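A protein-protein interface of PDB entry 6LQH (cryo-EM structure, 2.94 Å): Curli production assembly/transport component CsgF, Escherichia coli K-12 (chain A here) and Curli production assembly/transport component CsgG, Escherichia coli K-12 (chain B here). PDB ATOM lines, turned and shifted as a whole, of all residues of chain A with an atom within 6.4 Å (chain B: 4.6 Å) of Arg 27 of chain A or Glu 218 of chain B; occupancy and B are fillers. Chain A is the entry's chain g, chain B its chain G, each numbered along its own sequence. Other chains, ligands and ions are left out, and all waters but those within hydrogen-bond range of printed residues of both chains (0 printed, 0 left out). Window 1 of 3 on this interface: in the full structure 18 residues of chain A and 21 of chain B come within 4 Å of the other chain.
Along chain B the printed residues that touch a printed residue of chain A span positions 164 to 220.
The backbone carbonyl oxygen (O) of Gln 202 of chain B sits at hydrogen-bond distance from the backbone NH (N) of Asp 164 of chain B (2.9 Å).
The side-chain carboxylate (OE2) of Glu 200 of chain B lies within hydrogen-bond range of the side-chain amide nitrogen (NE2) of Gln 202 of chain B, at 2.6 Å.
The side-chain amide oxygen (OE1) of Gln 202 of chain B lies close to the side-chain carboxylate (OE1) of Glu 218 of chain B, 3.4 Å away.
O of Thr 23 of chain A sits at hydrogen-bond distance from NE2 of Gln 25 of chain A, at 3.1 Å.
The side-chain amide nitrogen (ND2) of Asn 37 of chain A sits close to the backbone carbonyl oxygen (O) of Arg 27 of chain A, at 3.3 Å.
Among the printed residues, pairs that only touch across the chains: Phe 24 of chain A with Gln 202 of chain B (3.5 Å), Phe 24 of chain A with Gly 220 of chain B (3.3 Å), Phe 26 of chain A with Glu 218 of chain B (3.5 Å) and Phe 31 of chain A with Glu 218 of chain B (3.97 Å).
The side-chain carboxylate (OD1) of Asp 164 of chain B is in salt-bridge range of the guanidinium group (NH2) of Arg 27 of chain A (3.0 Å).
The guanidinium group of Arg 27 of chain A is in salt-bridge range of the side-chain carboxylate of Glu 200 of chain B.
The side-chain amide nitrogen of Gln 202 of chain B sits at hydrogen-bond distance from the backbone carbonyl oxygen of Gln 25 of chain A, 3.3 Å away.
NE2 of Gln 202 of chain B sits close to NH1 of Arg 27 of chain A, 2.9 Å away.
OE1 of Glu 218 of chain B is in hydrogen-bond range of N of Arg 27 of chain A, at 2.8 Å.
Arg 27 of chain A touches just these residues of chain B: Asp 164, Glu 200, Gln 202 and Glu 218.
Glu 218 of chain B touches three residues of chain A.
Of the printed residues of chain B, Phe 26 of chain A touches Glu 218.
Printed residues of chain B within 4 Å of Phe 24 of chain A: Gln 202 (3.5 Å) and Gly 220 (3.3 Å).
Of the printed residues of chain A, Gln 202 of chain B touches Phe 24, Gln 25 and Arg 27.
Printed residues of chain B within 4 Å of Phe 31 of chain A: Glu 218.
Printed residues of chain A within 4 Å of Gly 220 of chain B: Phe 24 (3.3 Å).
Asn 34 of chain A touches none of the printed residues of chain B.
The nearest printed residue of chain B that does not touch Arg 27 of chain A is Ala 203 of chain B (6.6 Å).
The nearest residue of chain A that does not touch Glu 218 of chain B is Asn 28 of chain A (4.3 Å).
The nearest printed residue of chain B that does not touch Phe 31 of chain A is Gly 217 of chain B (4.4 Å).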
ATOM      1  N   THR A  23     -14.273 -24.006  16.570  1.00  0.00           N
ATOM      2  CA  THR A  23     -14.485 -24.708  15.318  1.00  0.00           C
ATOM      3  C   THR A  23     -13.129 -24.960  14.678  1.00  0.00           C
ATOM      4  O   THR A  23     -12.276 -24.067  14.659  1.00  0.00           O
ATOM      5  CB  THR A  23     -15.401 -23.899  14.397  1.00  0.00           C
ATOM      6  OG1 THR A  23     -16.705 -24.484  14.398  1.00  0.00           O
ATOM      7  CG2 THR A  23     -14.882 -23.890  12.967  1.00  0.00           C
ATOM      8  N   PHE A  24     -12.915 -26.183  14.204  1.00  0.00           N
ATOM      9  CA  PHE A  24     -11.649 -26.517  13.569  1.00  0.00           C
ATOM     10  C   PHE A  24     -11.535 -25.818  12.223  1.00  0.00           C
ATOM     11  O   PHE A  24     -12.463 -25.855  11.411  1.00  0.00           O
ATOM     12  CB  PHE A  24     -11.524 -28.028  13.390  1.00  0.00           C
ATOM     13  CG  PHE A  24     -10.454 -28.439  12.425  1.00  0.00           C
ATOM     14  CD1 PHE A  24      -9.131 -28.460  12.807  1.00  0.00           C
ATOM     15  CD2 PHE A  24     -10.773 -28.806  11.131  1.00  0.00           C
ATOM     16  CE1 PHE A  24      -8.149 -28.831  11.920  1.00  0.00           C
ATOM     17  CE2 PHE A  24      -9.791 -29.180  10.242  1.00  0.00           C
ATOM     18  CZ  PHE A  24      -8.479 -29.196  10.640  1.00  0.00           C
ATOM     19  N   GLN A  25     -10.400 -25.166  11.994  1.00  0.00           N
ATOM     20  CA  GLN A  25     -10.062 -24.618  10.691  1.00  0.00           C
ATOM     21  C   GLN A  25      -8.637 -25.019  10.355  1.00  0.00           C
ATOM     22  O   GLN A  25      -7.779 -25.076  11.241  1.00  0.00           O
ATOM     23  CB  GLN A  25     -10.205 -23.090  10.650  1.00  0.00           C
ATOM     24  CG  GLN A  25     -11.511 -22.542  11.209  1.00  0.00           C
ATOM     25  CD  GLN A  25     -11.313 -21.739  12.483  1.00  0.00           C
ATOM     26  OE1 GLN A  25     -10.184 -21.466  12.889  1.00  0.00           O
ATOM     27  NE2 GLN A  25     -12.413 -21.345  13.112  1.00  0.00           N
ATOM     28  N   PHE A  26      -8.394 -25.317   9.085  1.00  0.00           N
ATOM     29  CA  PHE A  26      -7.045 -25.617   8.634  1.00  0.00           C
ATOM     30  C   PHE A  26      -6.192 -24.353   8.625  1.00  0.00           C
ATOM     31  O   PHE A  26      -6.658 -23.265   8.276  1.00  0.00           O
ATOM     32  CB  PHE A  26      -7.079 -26.225   7.237  1.00  0.00           C
ATOM     33  CG  PHE A  26      -7.414 -27.682   7.216  1.00  0.00           C
ATOM     34  CD1 PHE A  26      -6.513 -28.618   7.675  1.00  0.00           C
ATOM     35  CD2 PHE A  26      -8.626 -28.118   6.725  1.00  0.00           C
ATOM     36  CE1 PHE A  26      -6.813 -29.955   7.652  1.00  0.00           C
ATOM     37  CE2 PHE A  26      -8.926 -29.458   6.696  1.00  0.00           C
ATOM     38  CZ  PHE A  26      -8.021 -30.375   7.162  1.00  0.00           C
ATOM     39  N   ARG A  27      -4.926 -24.502   9.017  1.00  0.00           N
ATOM     40  CA  ARG A  27      -4.001 -23.378   8.959  1.00  0.00           C
ATOM     41  C   ARG A  27      -3.487 -23.140   7.548  1.00  0.00           C
ATOM     42  O   ARG A  27      -3.237 -21.991   7.169  1.00  0.00           O
ATOM     43  CB  ARG A  27      -2.815 -23.611   9.892  1.00  0.00           C
ATOM     44  CG  ARG A  27      -3.185 -24.151  11.254  1.00  0.00           C
ATOM     45  CD  ARG A  27      -3.807 -23.095  12.126  1.00  0.00           C
ATOM     46  NE  ARG A  27      -3.729 -23.480  13.527  1.00  0.00           N
ATOM     47  CZ  ARG A  27      -4.778 -23.632  14.322  1.00  0.00           C
ATOM     48  NH1 ARG A  27      -6.000 -23.419  13.856  1.00  0.00           N
ATOM     49  NH2 ARG A  27      -4.604 -23.987  15.586  1.00  0.00           N
ATOM     50  N   ASN A  28      -3.314 -24.199   6.766  1.00  0.00           N
ATOM     51  CA  ASN A  28      -2.831 -24.031   5.409  1.00  0.00           C
ATOM     52  C   ASN A  28      -3.934 -23.492   4.504  1.00  0.00           C
ATOM     53  O   ASN A  28      -5.098 -23.877   4.636  1.00  0.00           O
ATOM     54  CB  ASN A  28      -2.334 -25.359   4.841  1.00  0.00           C
ATOM     55  CG  ASN A  28      -1.023 -25.808   5.441  1.00  0.00           C
ATOM     56  OD1 ASN A  28      -0.366 -25.063   6.162  1.00  0.00           O
ATOM     57  ND2 ASN A  28      -0.619 -27.027   5.121  1.00  0.00           N
ATOM     58  N   PRO A  29      -3.588 -22.590   3.586  1.00  0.00           N
ATOM     59  CA  PRO A  29      -4.510 -22.294   2.485  1.00  0.00           C
ATOM     60  C   PRO A  29      -4.704 -23.483   1.574  1.00  0.00           C
ATOM     61  O   PRO A  29      -5.820 -23.711   1.092  1.00  0.00           O
ATOM     62  CB  PRO A  29      -3.831 -21.130   1.759  1.00  0.00           C
ATOM     63  CG  PRO A  29      -2.416 -21.252   2.111  1.00  0.00           C
ATOM     64  CD  PRO A  29      -2.355 -21.799   3.497  1.00  0.00           C
ATOM     65  N   ASN A  30      -3.642 -24.243   1.316  1.00  0.00           N
ATOM     66  CA  ASN A  30      -3.815 -25.578   0.773  1.00  0.00           C
ATOM     67  C   ASN A  30      -4.710 -26.371   1.706  1.00  0.00           C
ATOM     68  O   ASN A  30      -4.493 -26.408   2.918  1.00  0.00           O
ATOM     69  CB  ASN A  30      -2.468 -26.281   0.619  1.00  0.00           C
ATOM     70  CG  ASN A  30      -1.637 -25.709  -0.502  1.00  0.00           C
ATOM     71  OD1 ASN A  30      -2.166 -25.139  -1.453  1.00  0.00           O
ATOM     72  ND2 ASN A  30      -0.323 -25.859  -0.398  1.00  0.00           N
ATOM     73  N   PHE A  31      -5.734 -26.991   1.134  1.00  0.00           N
ATOM     74  CA  PHE A  31      -6.704 -27.780   1.881  1.00  0.00           C
ATOM     75  C   PHE A  31      -7.222 -27.095   3.145  1.00  0.00           C
ATOM     76  O   PHE A  31      -6.908 -27.513   4.257  1.00  0.00           O
ATOM     77  CB  PHE A  31      -6.171 -29.196   2.195  1.00  0.00           C
ATOM     78  CG  PHE A  31      -4.815 -29.273   2.868  1.00  0.00           C
ATOM     79  CD1 PHE A  31      -4.689 -29.171   4.244  1.00  0.00           C
ATOM     80  CD2 PHE A  31      -3.684 -29.559   2.129  1.00  0.00           C
ATOM     81  CE1 PHE A  31      -3.462 -29.274   4.852  1.00  0.00           C
ATOM     82  CE2 PHE A  31      -2.455 -29.668   2.740  1.00  0.00           C
ATOM     83  CZ  PHE A  31      -2.345 -29.526   4.101  1.00  0.00           C
ATOM     84  N   GLY A  32      -8.026 -26.043   2.993  1.00  0.00           N
ATOM     85  CA  GLY A  32      -8.765 -25.573   4.148  1.00  0.00           C
ATOM     86  C   GLY A  32      -9.043 -24.097   4.351  1.00  0.00           C
ATOM     87  O   GLY A  32      -9.640 -23.730   5.367  1.00  0.00           O
ATOM     88  N   ASN A  34      -7.866 -20.512   4.590  1.00  0.00           N
ATOM     89  CA  ASN A  34      -7.349 -19.182   4.892  1.00  0.00           C
ATOM     90  C   ASN A  34      -6.121 -18.911   4.036  1.00  0.00           C
ATOM     91  O   ASN A  34      -5.070 -19.530   4.252  1.00  0.00           O
ATOM     92  CB  ASN A  34      -7.020 -19.033   6.378  1.00  0.00           C
ATOM     93  CG  ASN A  34      -6.878 -17.576   6.800  1.00  0.00           C
ATOM     94  OD1 ASN A  34      -6.593 -16.704   5.985  1.00  0.00           O
ATOM     95  ND2 ASN A  34      -7.087 -17.311   8.082  1.00  0.00           N
ATOM     96  N   ASN A  37      -2.293 -17.163   5.193  1.00  0.00           N
ATOM     97  CA  ASN A  37      -1.265 -17.917   5.905  1.00  0.00           C
ATOM     98  C   ASN A  37      -0.181 -18.415   4.961  1.00  0.00           C
ATOM     99  O   ASN A  37       0.966 -18.604   5.376  1.00  0.00           O
ATOM    100  CB  ASN A  37      -1.886 -19.094   6.656  1.00  0.00           C
ATOM    101  CG  ASN A  37      -2.769 -18.657   7.797  1.00  0.00           C
ATOM    102  OD1 ASN A  37      -2.293 -18.144   8.806  1.00  0.00           O
ATOM    103  ND2 ASN A  37      -4.066 -18.868   7.648  1.00  0.00           N
ATOM    104  N   GLY A  38      -0.528 -18.641   3.694  1.00  0.00           N
ATOM    105  CA  GLY A  38       0.392 -19.318   2.795  1.00  0.00           C
ATOM    106  C   GLY A  38       1.625 -18.499   2.468  1.00  0.00           C
ATOM    107  O   GLY A  38       2.720 -19.046   2.312  1.00  0.00           O
ATOM    108  N   LEU A  41       3.823 -19.022   5.293  1.00  0.00           N
ATOM    109  CA  LEU A  41       4.182 -20.428   5.423  1.00  0.00           C
ATOM    110  C   LEU A  41       5.292 -20.807   4.459  1.00  0.00           C
ATOM    111  O   LEU A  41       6.279 -21.439   4.855  1.00  0.00           O
ATOM    112  CB  LEU A  41       2.952 -21.297   5.185  1.00  0.00           C
ATOM    113  CG  LEU A  41       2.141 -21.626   6.432  1.00  0.00           C
ATOM    114  CD1 LEU A  41       0.802 -22.192   6.035  1.00  0.00           C
ATOM    115  CD2 LEU A  41       2.898 -22.601   7.313  1.00  0.00           C
ATOM    116  N   ASP B 164      -0.069 -27.142  18.564  1.00  0.00           N
ATOM    117  CA  ASP B 164      -0.640 -26.239  19.547  1.00  0.00           C
ATOM    118  C   ASP B 164      -1.864 -26.847  20.203  1.00  0.00           C
ATOM    119  O   ASP B 164      -2.528 -27.727  19.654  1.00  0.00           O
ATOM    120  CB  ASP B 164      -1.052 -24.911  18.943  1.00  0.00           C
ATOM    121  CG  ASP B 164      -2.376 -24.992  18.218  1.00  0.00           C
ATOM    122  OD1 ASP B 164      -2.380 -25.372  17.031  1.00  0.00           O
ATOM    123  OD2 ASP B 164      -3.418 -24.680  18.830  1.00  0.00           O
ATOM    124  N   GLU B 200      -8.968 -27.560  21.737  1.00  0.00           N
ATOM    125  CA  GLU B 200      -8.608 -27.681  20.329  1.00  0.00           C
ATOM    126  C   GLU B 200      -7.131 -28.014  20.242  1.00  0.00           C
ATOM    127  O   GLU B 200      -6.308 -27.281  20.784  1.00  0.00           O
ATOM    128  CB  GLU B 200      -8.909 -26.391  19.597  1.00  0.00           C
ATOM    129  CG  GLU B 200      -8.260 -26.290  18.248  1.00  0.00           C
ATOM    130  CD  GLU B 200      -8.861 -25.189  17.412  1.00  0.00           C
ATOM    131  OE1 GLU B 200      -9.699 -24.437  17.945  1.00  0.00           O
ATOM    132  OE2 GLU B 200      -8.496 -25.074  16.223  1.00  0.00           O
ATOM    133  N   GLN B 202      -4.060 -28.948  17.477  1.00  0.00           N
ATOM    134  CA  GLN B 202      -3.645 -29.032  16.088  1.00  0.00           C
ATOM    135  C   GLN B 202      -2.168 -29.367  16.016  1.00  0.00           C
ATOM    136  O   GLN B 202      -1.402 -29.101  16.939  1.00  0.00           O
ATOM    137  CB  GLN B 202      -3.922 -27.734  15.333  1.00  0.00           C
ATOM    138  CG  GLN B 202      -5.334 -27.245  15.489  1.00  0.00           C
ATOM    139  CD  GLN B 202      -5.911 -26.735  14.194  1.00  0.00           C
ATOM    140  OE1 GLN B 202      -5.332 -26.931  13.127  1.00  0.00           O
ATOM    141  NE2 GLN B 202      -7.063 -26.080  14.276  1.00  0.00           N
ATOM    142  N   ALA B 203      -1.782 -29.964  14.898  1.00  0.00           N
ATOM    143  CA  ALA B 203      -0.392 -30.264  14.617  1.00  0.00           C
ATOM    144  C   ALA B 203      -0.192 -30.133  13.118  1.00  0.00           C
ATOM    145  O   ALA B 203      -1.128 -30.288  12.337  1.00  0.00           O
ATOM    146  CB  ALA B 203      -0.004 -31.658  15.110  1.00  0.00           C
ATOM    147  N   GLY B 204       1.036 -29.843  12.720  1.00  0.00           N
ATOM    148  CA  GLY B 204       1.296 -29.598  11.319  1.00  0.00           C
ATOM    149  C   GLY B 204       2.755 -29.663  10.931  1.00  0.00           C
ATOM    150  O   GLY B 204       3.639 -29.389  11.741  1.00  0.00           O
ATOM    151  N   GLY B 217       1.371 -31.026   5.988  1.00  0.00           N
ATOM    152  CA  GLY B 217       0.496 -31.940   6.682  1.00  0.00           C
ATOM    153  C   GLY B 217      -0.142 -31.260   7.865  1.00  0.00           C
ATOM    154  O   GLY B 217       0.446 -30.355   8.452  1.00  0.00           O
ATOM    155  N   GLU B 218      -1.335 -31.696   8.234  1.00  0.00           N
ATOM    156  CA  GLU B 218      -2.081 -31.031   9.284  1.00  0.00           C
ATOM    157  C   GLU B 218      -3.056 -32.024   9.883  1.00  0.00           C
ATOM    158  O   GLU B 218      -3.726 -32.753   9.154  1.00  0.00           O
ATOM    159  CB  GLU B 218      -2.830 -29.820   8.732  1.00  0.00           C
ATOM    160  CG  GLU B 218      -3.781 -29.189   9.708  1.00  0.00           C
ATOM    161  CD  GLU B 218      -3.266 -27.888  10.282  1.00  0.00           C
ATOM    162  OE1 GLU B 218      -3.944 -26.865  10.073  1.00  0.00           O
ATOM    163  OE2 GLU B 218      -2.200 -27.877  10.934  1.00  0.00           O
ATOM    164  N   VAL B 219      -3.114 -32.062  11.207  1.00  0.00           N
ATOM    165  CA  VAL B 219      -4.074 -32.880  11.932  1.00  0.00           C
ATOM    166  C   VAL B 219      -4.712 -32.006  12.993  1.00  0.00           C
ATOM    167  O   VAL B 219      -4.015 -31.407  13.812  1.00  0.00           O
ATOM    168  CB  VAL B 219      -3.413 -34.110  12.581  1.00  0.00           C
ATOM    169  CG1 VAL B 219      -4.408 -34.841  13.448  1.00  0.00           C
ATOM    170  CG2 VAL B 219      -2.854 -35.029  11.534  1.00  0.00           C
ATOM    171  N   GLY B 220      -6.032 -31.925  12.984  1.00  0.00           N
ATOM    172  CA  GLY B 220      -6.719 -31.059  13.912  1.00  0.00           C
ATOM    173  C   GLY B 220      -7.848 -31.786  14.604  1.00  0.00           C
ATOM    174  O   GLY B 220      -8.451 -32.713  14.064  1.00  0.00           O
